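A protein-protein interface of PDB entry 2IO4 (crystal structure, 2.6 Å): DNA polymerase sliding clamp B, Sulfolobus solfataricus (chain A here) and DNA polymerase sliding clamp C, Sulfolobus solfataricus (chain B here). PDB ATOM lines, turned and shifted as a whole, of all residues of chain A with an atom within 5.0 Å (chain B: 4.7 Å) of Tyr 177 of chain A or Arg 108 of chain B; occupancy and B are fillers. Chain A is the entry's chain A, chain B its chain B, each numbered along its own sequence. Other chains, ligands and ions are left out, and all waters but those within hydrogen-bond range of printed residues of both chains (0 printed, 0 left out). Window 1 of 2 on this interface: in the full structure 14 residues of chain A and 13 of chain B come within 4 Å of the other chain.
NH1 of Arg 82 of chain B lies within hydrogen-bond range of O of Val 145 of chain A (3.4 Å). NE of Arg 82 of chain B is in salt-bridge range of OD1 of Asp 149 of chain A, at 2.9 Å. The side-chain carboxylate of Asp 149 of chain A lies within salt-bridge range of the guanidinium group of Arg 108 of chain B, at 2.8 Å. O of Val 178 of chain A lies within hydrogen-bond range of N of Ser 109 of chain B (2.8 Å).
OH of Tyr 177 of chain A lies within hydrogen-bond range of OD2 of Asp 149 of chain A. The backbone carbonyl oxygen of Ile 168 of chain A lies within hydrogen-bond range of the backbone NH of Ala 179 of chain A, at 2.9 Å. The guanidinium group (NH2) of Arg 108 of chain B is in salt-bridge range of the side-chain carboxylate (OD1) of Asp 87 of chain B (2.8 Å). The backbone carbonyl oxygen of Leu 100 of chain B lies within hydrogen-bond range of the backbone NH of Phe 110 of chain B. The side-chain hydroxyl of Thr 101 of chain B sits at hydrogen-bond distance from the side-chain hydroxyl of Ser 109 of chain B (2.8 Å). The backbone carbonyl oxygen (O) of Phe 102 of chain B is in hydrogen-bond range of the backbone NH (N) of Arg 108 of chain B, at 2.6 Å.
CG2 of Val 145 of chain A touches CD2 of Leu 84 of chain B, at 3.9 Å. Val 145 of chain A touches Arg 108 of chain B (CG1 to NH1, 3.3 Å). Phe 110 of chain B touches Asp 149 of chain A. Phe 110 of chain B touches Val 153 of chain A. Phe 110 of chain B touches Arg 176 of chain A (CA to O, 3.5 Å). Tyr 177 of chain A touches Arg 108 of chain B (CE1 to CB, 3.9 Å). Tyr 177 of chain A touches Ser 109 of chain B. CD1 of Tyr 177 of chain A touches CE2 of Phe 110 of chain B, 3.4 Å away. Arg 108 of chain B touches Val 178 of chain A (CA to O, 3.5 Å). CA of Ala 179 of chain A touches O of Thr 107 of chain B (3.5 Å).
Of the printed residues of chain B, Tyr 177 of chain A touches Arg 108 (3.9 Å), Ser 109 (3.1 Å) and Phe 110 (3.4 Å). Arg 108 of chain B touches four residues of chain A. Printed residues of chain A within 4 Å of Phe 110 of chain B: Asp 149, Val 153, Arg 176 and Tyr 177. Printed residues of chain B within 4 Å of Ala 179 of chain A: Thr 107. The nearest printed residue of chain B that does not touch Tyr 177 of chain A is Phe 106 of chain B (4.7 Å). The nearest printed residue of chain B that does not touch Asp 149 of chain A is Phe 106 of chain B (5.4 Å).
Printed residues of chain B that touch a printed residue of chain A: Arg 82, Leu 84, Phe 106, Thr 107, Arg 108, Ser 109 and Phe 110. Hydrophobic or aromatic side chains of chain B within 4 Å of the printed part of chain A: Leu 84, Phe 106 and Phe 110. Among the printed residues, 15 pairs touch across the chains.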
ATOM      1  N   VAL A 145      20.492   3.605 -16.316  1.00  0.00           N
ATOM      2  CA  VAL A 145      21.352   2.499 -16.716  1.00  0.00           C
ATOM      3  C   VAL A 145      21.502   1.511 -15.556  1.00  0.00           C
ATOM      4  O   VAL A 145      21.475   0.293 -15.756  1.00  0.00           O
ATOM      5  CB  VAL A 145      22.734   3.015 -17.194  1.00  0.00           C
ATOM      6  CG1 VAL A 145      23.703   1.872 -17.410  1.00  0.00           C
ATOM      7  CG2 VAL A 145      22.580   3.845 -18.472  1.00  0.00           C
ATOM      8  N   ILE A 146      21.630   2.050 -14.346  1.00  0.00           N
ATOM      9  CA  ILE A 146      21.809   1.233 -13.146  1.00  0.00           C
ATOM     10  C   ILE A 146      20.520   0.489 -12.779  1.00  0.00           C
ATOM     11  O   ILE A 146      20.558  -0.701 -12.449  1.00  0.00           O
ATOM     12  CB  ILE A 146      22.304   2.074 -11.943  1.00  0.00           C
ATOM     13  CG1 ILE A 146      23.698   2.662 -12.220  1.00  0.00           C
ATOM     14  CG2 ILE A 146      22.303   1.234 -10.662  1.00  0.00           C
ATOM     15  CD1 ILE A 146      24.113   3.820 -11.255  1.00  0.00           C
ATOM     16  N   ASP A 149      20.313  -2.364 -15.097  1.00  0.00           N
ATOM     17  CA  ASP A 149      21.363  -3.334 -14.812  1.00  0.00           C
ATOM     18  C   ASP A 149      20.986  -4.284 -13.672  1.00  0.00           C
ATOM     19  O   ASP A 149      20.940  -5.508 -13.880  1.00  0.00           O
ATOM     20  CB  ASP A 149      22.673  -2.622 -14.489  1.00  0.00           C
ATOM     21  CG  ASP A 149      23.335  -2.051 -15.717  1.00  0.00           C
ATOM     22  OD1 ASP A 149      22.813  -2.286 -16.836  1.00  0.00           O
ATOM     23  OD2 ASP A 149      24.371  -1.365 -15.555  1.00  0.00           O
ATOM     24  N   VAL A 150      20.710  -3.721 -12.489  1.00  0.00           N
ATOM     25  CA  VAL A 150      20.372  -4.521 -11.302  1.00  0.00           C
ATOM     26  C   VAL A 150      19.091  -5.356 -11.476  1.00  0.00           C
ATOM     27  O   VAL A 150      19.057  -6.524 -11.074  1.00  0.00           O
ATOM     28  CB  VAL A 150      20.340  -3.691  -9.980  1.00  0.00           C
ATOM     29  CG1 VAL A 150      21.684  -3.028  -9.729  1.00  0.00           C
ATOM     30  CG2 VAL A 150      19.248  -2.643  -9.999  1.00  0.00           C
ATOM     31  N   VAL A 153      19.472  -8.656 -13.006  1.00  0.00           N
ATOM     32  CA  VAL A 153      20.225  -9.652 -12.235  1.00  0.00           C
ATOM     33  C   VAL A 153      19.581 -10.046 -10.889  1.00  0.00           C
ATOM     34  O   VAL A 153      19.759 -11.175 -10.420  1.00  0.00           O
ATOM     35  CB  VAL A 153      21.729  -9.247 -12.076  1.00  0.00           C
ATOM     36  CG1 VAL A 153      22.507 -10.336 -11.394  1.00  0.00           C
ATOM     37  CG2 VAL A 153      22.363  -8.966 -13.441  1.00  0.00           C
ATOM     38  N   ILE A 168      27.863  -0.496  -6.300  1.00  0.00           N
ATOM     39  CA  ILE A 168      26.484  -0.956  -6.433  1.00  0.00           C
ATOM     40  C   ILE A 168      26.486  -2.408  -6.895  1.00  0.00           C
ATOM     41  O   ILE A 168      27.112  -2.731  -7.902  1.00  0.00           O
ATOM     42  CB  ILE A 168      25.704  -0.083  -7.446  1.00  0.00           C
ATOM     43  CG1 ILE A 168      25.698   1.381  -6.987  1.00  0.00           C
ATOM     44  CG2 ILE A 168      24.278  -0.618  -7.651  1.00  0.00           C
ATOM     45  CD1 ILE A 168      24.897   2.310  -7.863  1.00  0.00           C
ATOM     46  N   GLU A 169      25.787  -3.272  -6.157  1.00  0.00           N
ATOM     47  CA  GLU A 169      25.743  -4.703  -6.478  1.00  0.00           C
ATOM     48  C   GLU A 169      24.358  -5.354  -6.367  1.00  0.00           C
ATOM     49  O   GLU A 169      23.488  -4.866  -5.635  1.00  0.00           O
ATOM     50  CB  GLU A 169      26.783  -5.476  -5.662  1.00  0.00           C
ATOM     51  CG  GLU A 169      26.744  -5.231  -4.159  1.00  0.00           C
ATOM     52  CD  GLU A 169      27.997  -5.738  -3.458  1.00  0.00           C
ATOM     53  OE1 GLU A 169      28.689  -6.628  -4.014  1.00  0.00           O
ATOM     54  OE2 GLU A 169      28.290  -5.242  -2.346  1.00  0.00           O
ATOM     55  N   ALA A 170      24.169  -6.441  -7.127  1.00  0.00           N
ATOM     56  CA  ALA A 170      22.948  -7.265  -7.093  1.00  0.00           C
ATOM     57  C   ALA A 170      23.207  -8.701  -7.591  1.00  0.00           C
ATOM     58  O   ALA A 170      24.254  -8.981  -8.176  1.00  0.00           O
ATOM     59  CB  ALA A 170      21.821  -6.601  -7.890  1.00  0.00           C
ATOM     60  N   LYS A 175      24.774 -15.464 -10.430  1.00  0.00           N
ATOM     61  CA  LYS A 175      24.808 -14.424 -11.468  1.00  0.00           C
ATOM     62  C   LYS A 175      24.795 -13.047 -10.815  1.00  0.00           C
ATOM     63  O   LYS A 175      23.880 -12.731 -10.049  1.00  0.00           O
ATOM     64  CB  LYS A 175      23.601 -14.554 -12.411  1.00  0.00           C
ATOM     65  CG  LYS A 175      23.507 -15.878 -13.180  1.00  0.00           C
ATOM     66  CD  LYS A 175      22.252 -15.896 -14.062  1.00  0.00           C
ATOM     67  CE  LYS A 175      22.114 -17.291 -14.748  1.00  0.00           C
ATOM     68  NZ  LYS A 175      20.813 -17.310 -15.509  1.00  0.00           N
ATOM     69  N   ARG A 176      25.791 -12.220 -11.134  1.00  0.00           N
ATOM     70  CA  ARG A 176      26.056 -11.016 -10.343  1.00  0.00           C
ATOM     71  C   ARG A 176      26.332  -9.744 -11.164  1.00  0.00           C
ATOM     72  O   ARG A 176      26.595  -9.819 -12.365  1.00  0.00           O
ATOM     73  CB  ARG A 176      27.210 -11.311  -9.387  1.00  0.00           C
ATOM     74  CG  ARG A 176      26.890 -11.001  -7.941  1.00  0.00           C
ATOM     75  CD  ARG A 176      27.615 -11.947  -6.998  1.00  0.00           C
ATOM     76  NE  ARG A 176      29.073 -11.891  -7.148  1.00  0.00           N
ATOM     77  CZ  ARG A 176      29.856 -10.925  -6.657  1.00  0.00           C
ATOM     78  NH1 ARG A 176      29.331  -9.901  -5.990  1.00  0.00           N
ATOM     79  NH2 ARG A 176      31.175 -10.981  -6.840  1.00  0.00           N
ATOM     80  N   TYR A 177      26.259  -8.584 -10.503  1.00  0.00           N
ATOM     81  CA  TYR A 177      26.513  -7.269 -11.120  1.00  0.00           C
ATOM     82  C   TYR A 177      27.218  -6.315 -10.157  1.00  0.00           C
ATOM     83  O   TYR A 177      26.779  -6.161  -9.012  1.00  0.00           O
ATOM     84  CB  TYR A 177      25.191  -6.629 -11.569  1.00  0.00           C
ATOM     85  CG  TYR A 177      25.290  -5.168 -11.990  1.00  0.00           C
ATOM     86  CD1 TYR A 177      25.924  -4.807 -13.188  1.00  0.00           C
ATOM     87  CD2 TYR A 177      24.738  -4.154 -11.196  1.00  0.00           C
ATOM     88  CE1 TYR A 177      26.014  -3.478 -13.581  1.00  0.00           C
ATOM     89  CE2 TYR A 177      24.822  -2.813 -11.578  1.00  0.00           C
ATOM     90  CZ  TYR A 177      25.464  -2.486 -12.769  1.00  0.00           C
ATOM     91  OH  TYR A 177      25.540  -1.170 -13.163  1.00  0.00           O
ATOM     92  N   VAL A 178      28.291  -5.666 -10.631  1.00  0.00           N
ATOM     93  CA  VAL A 178      28.950  -4.601  -9.856  1.00  0.00           C
ATOM     94  C   VAL A 178      29.289  -3.361 -10.692  1.00  0.00           C
ATOM     95  O   VAL A 178      29.962  -3.458 -11.720  1.00  0.00           O
ATOM     96  CB  VAL A 178      30.217  -5.107  -9.087  1.00  0.00           C
ATOM     97  CG1 VAL A 178      31.349  -5.498 -10.044  1.00  0.00           C
ATOM     98  CG2 VAL A 178      30.705  -4.049  -8.100  1.00  0.00           C
ATOM     99  N   ALA A 179      28.823  -2.200 -10.236  1.00  0.00           N
ATOM    100  CA  ALA A 179      29.145  -0.920 -10.859  1.00  0.00           C
ATOM    101  C   ALA A 179      29.900  -0.014  -9.897  1.00  0.00           C
ATOM    102  O   ALA A 179      29.577   0.068  -8.696  1.00  0.00           O
ATOM    103  CB  ALA A 179      27.880  -0.219 -11.329  1.00  0.00           C
ATOM    104  N   ARG B  82      22.870  -4.600 -22.646  1.00  0.00           N
ATOM    105  CA  ARG B  82      23.069  -3.442 -21.772  1.00  0.00           C
ATOM    106  C   ARG B  82      24.246  -2.573 -22.231  1.00  0.00           C
ATOM    107  O   ARG B  82      24.621  -1.623 -21.543  1.00  0.00           O
ATOM    108  CB  ARG B  82      23.304  -3.876 -20.313  1.00  0.00           C
ATOM    109  CG  ARG B  82      22.421  -5.007 -19.768  1.00  0.00           C
ATOM    110  CD  ARG B  82      20.982  -4.579 -19.500  1.00  0.00           C
ATOM    111  NE  ARG B  82      20.923  -3.272 -18.855  1.00  0.00           N
ATOM    112  CZ  ARG B  82      20.448  -2.168 -19.433  1.00  0.00           C
ATOM    113  NH1 ARG B  82      20.456  -1.030 -18.762  1.00  0.00           N
ATOM    114  NH2 ARG B  82      19.963  -2.195 -20.678  1.00  0.00           N
ATOM    115  N   VAL B  83      24.832  -2.911 -23.381  1.00  0.00           N
ATOM    116  CA  VAL B  83      25.946  -2.140 -23.964  1.00  0.00           C
ATOM    117  C   VAL B  83      25.534  -0.686 -24.202  1.00  0.00           C
ATOM    118  O   VAL B  83      24.376  -0.412 -24.515  1.00  0.00           O
ATOM    119  CB  VAL B  83      26.501  -2.807 -25.274  1.00  0.00           C
ATOM    120  CG1 VAL B  83      25.377  -3.125 -26.265  1.00  0.00           C
ATOM    121  CG2 VAL B  83      27.616  -1.937 -25.941  1.00  0.00           C
ATOM    122  N   LEU B  84      26.478   0.240 -24.058  1.00  0.00           N
ATOM    123  CA  LEU B  84      26.134   1.657 -24.086  1.00  0.00           C
ATOM    124  C   LEU B  84      26.872   2.483 -25.150  1.00  0.00           C
ATOM    125  O   LEU B  84      27.082   3.690 -24.971  1.00  0.00           O
ATOM    126  CB  LEU B  84      26.313   2.263 -22.690  1.00  0.00           C
ATOM    127  CG  LEU B  84      25.189   3.141 -22.133  1.00  0.00           C
ATOM    128  CD1 LEU B  84      23.915   2.297 -21.879  1.00  0.00           C
ATOM    129  CD2 LEU B  84      25.690   3.774 -20.828  1.00  0.00           C
ATOM    130  N   ASP B  87      30.724   2.444 -24.736  1.00  0.00           N
ATOM    131  CA  ASP B  87      31.311   1.507 -23.814  1.00  0.00           C
ATOM    132  C   ASP B  87      32.298   0.644 -24.561  1.00  0.00           C
ATOM    133  O   ASP B  87      31.957   0.028 -25.580  1.00  0.00           O
ATOM    134  CB  ASP B  87      30.236   0.626 -23.177  1.00  0.00           C
ATOM    135  CG  ASP B  87      29.686   1.211 -21.893  1.00  0.00           C
ATOM    136  OD1 ASP B  87      28.701   0.652 -21.379  1.00  0.00           O
ATOM    137  OD2 ASP B  87      30.235   2.217 -21.389  1.00  0.00           O
ATOM    138  N   LEU B 100      31.972  -9.882 -17.999  1.00  0.00           N
ATOM    139  CA  LEU B 100      31.815  -8.959 -19.109  1.00  0.00           C
ATOM    140  C   LEU B 100      31.800  -7.557 -18.517  1.00  0.00           C
ATOM    141  O   LEU B 100      30.953  -7.249 -17.672  1.00  0.00           O
ATOM    142  CB  LEU B 100      30.506  -9.252 -19.847  1.00  0.00           C
ATOM    143  CG  LEU B 100      30.358 -10.657 -20.458  1.00  0.00           C
ATOM    144  CD1 LEU B 100      28.982 -11.253 -20.209  1.00  0.00           C
ATOM    145  CD2 LEU B 100      30.680 -10.667 -21.947  1.00  0.00           C
ATOM    146  N   THR B 101      32.740  -6.713 -18.935  1.00  0.00           N
ATOM    147  CA  THR B 101      32.901  -5.404 -18.304  1.00  0.00           C
ATOM    148  C   THR B 101      32.685  -4.238 -19.256  1.00  0.00           C
ATOM    149  O   THR B 101      33.452  -4.035 -20.201  1.00  0.00           O
ATOM    150  CB  THR B 101      34.262  -5.275 -17.566  1.00  0.00           C
ATOM    151  OG1 THR B 101      34.318  -6.239 -16.505  1.00  0.00           O
ATOM    152  CG2 THR B 101      34.447  -3.877 -16.965  1.00  0.00           C
ATOM    153  N   PHE B 102      31.632  -3.473 -18.988  1.00  0.00           N
ATOM    154  CA  PHE B 102      31.359  -2.248 -19.734  1.00  0.00           C
ATOM    155  C   PHE B 102      32.059  -1.087 -19.041  1.00  0.00           C
ATOM    156  O   PHE B 102      31.870  -0.847 -17.845  1.00  0.00           O
ATOM    157  CB  PHE B 102      29.848  -1.981 -19.878  1.00  0.00           C
ATOM    158  CG  PHE B 102      29.080  -3.100 -20.546  1.00  0.00           C
ATOM    159  CD1 PHE B 102      27.999  -3.699 -19.902  1.00  0.00           C
ATOM    160  CD2 PHE B 102      29.430  -3.554 -21.817  1.00  0.00           C
ATOM    161  CE1 PHE B 102      27.279  -4.733 -20.510  1.00  0.00           C
ATOM    162  CE2 PHE B 102      28.712  -4.587 -22.434  1.00  0.00           C
ATOM    163  CZ  PHE B 102      27.639  -5.179 -21.777  1.00  0.00           C
ATOM    164  N   PHE B 106      31.110   5.277 -17.391  1.00  0.00           N
ATOM    165  CA  PHE B 106      31.504   4.701 -16.091  1.00  0.00           C
ATOM    166  C   PHE B 106      31.662   3.168 -16.209  1.00  0.00           C
ATOM    167  O   PHE B 106      31.312   2.583 -17.238  1.00  0.00           O
ATOM    168  CB  PHE B 106      30.540   5.102 -14.963  1.00  0.00           C
ATOM    169  CG  PHE B 106      29.157   4.548 -15.113  1.00  0.00           C
ATOM    170  CD1 PHE B 106      28.284   5.058 -16.078  1.00  0.00           C
ATOM    171  CD2 PHE B 106      28.725   3.519 -14.276  1.00  0.00           C
ATOM    172  CE1 PHE B 106      27.001   4.538 -16.216  1.00  0.00           C
ATOM    173  CE2 PHE B 106      27.444   2.999 -14.399  1.00  0.00           C
ATOM    174  CZ  PHE B 106      26.578   3.507 -15.369  1.00  0.00           C
ATOM    175  N   THR B 107      32.190   2.527 -15.164  1.00  0.00           N
ATOM    176  CA  THR B 107      32.550   1.103 -15.224  1.00  0.00           C
ATOM    177  C   THR B 107      31.512   0.179 -14.580  1.00  0.00           C
ATOM    178  O   THR B 107      31.066   0.406 -13.457  1.00  0.00           O
ATOM    179  CB  THR B 107      33.957   0.849 -14.610  1.00  0.00           C
ATOM    180  OG1 THR B 107      34.897   1.760 -15.200  1.00  0.00           O
ATOM    181  CG2 THR B 107      34.436  -0.570 -14.895  1.00  0.00           C
ATOM    182  N   ARG B 108      31.143  -0.870 -15.308  1.00  0.00           N
ATOM    183  CA  ARG B 108      30.135  -1.831 -14.866  1.00  0.00           C
ATOM    184  C   ARG B 108      30.540  -3.242 -15.292  1.00  0.00           C
ATOM    185  O   ARG B 108      31.055  -3.433 -16.397  1.00  0.00           O
ATOM    186  CB  ARG B 108      28.782  -1.505 -15.495  1.00  0.00           C
ATOM    187  CG  ARG B 108      28.522  -0.025 -15.738  1.00  0.00           C
ATOM    188  CD  ARG B 108      27.210   0.173 -16.471  1.00  0.00           C
ATOM    189  NE  ARG B 108      27.341   0.058 -17.916  1.00  0.00           N
ATOM    190  CZ  ARG B 108      26.410  -0.469 -18.704  1.00  0.00           C
ATOM    191  NH1 ARG B 108      25.294  -0.959 -18.182  1.00  0.00           N
ATOM    192  NH2 ARG B 108      26.606  -0.540 -20.012  1.00  0.00           N
ATOM    193  N   SER B 109      30.289  -4.227 -14.429  1.00  0.00           N
ATOM    194  CA  SER B 109      30.633  -5.626 -14.716  1.00  0.00           C
ATOM    195  C   SER B 109      29.457  -6.570 -14.474  1.00  0.00           C
ATOM    196  O   SER B 109      28.645  -6.337 -13.577  1.00  0.00           O
ATOM    197  CB  SER B 109      31.837  -6.072 -13.879  1.00  0.00           C
ATOM    198  OG  SER B 109      33.002  -5.322 -14.194  1.00  0.00           O
ATOM    199  N   PHE B 110      29.369  -7.628 -15.284  1.00  0.00           N
ATOM    200  CA  PHE B 110      28.366  -8.681 -15.109  1.00  0.00           C
ATOM    201  C   PHE B 110      29.033 -10.042 -15.020  1.00  0.00           C
ATOM    202  O   PHE B 110      29.841 -10.408 -15.877  1.00  0.00           O
ATOM    203  CB  PHE B 110      27.371  -8.691 -16.267  1.00  0.00           C
ATOM    204  CG  PHE B 110      26.442  -7.507 -16.287  1.00  0.00           C
ATOM    205  CD1 PHE B 110      26.785  -6.349 -16.981  1.00  0.00           C
ATOM    206  CD2 PHE B 110      25.219  -7.554 -15.617  1.00  0.00           C
ATOM    207  CE1 PHE B 110      25.929  -5.259 -17.005  1.00  0.00           C
ATOM    208  CE2 PHE B 110      24.355  -6.473 -15.635  1.00  0.00           C
ATOM    209  CZ  PHE B 110      24.708  -5.320 -16.332  1.00  0.00           C
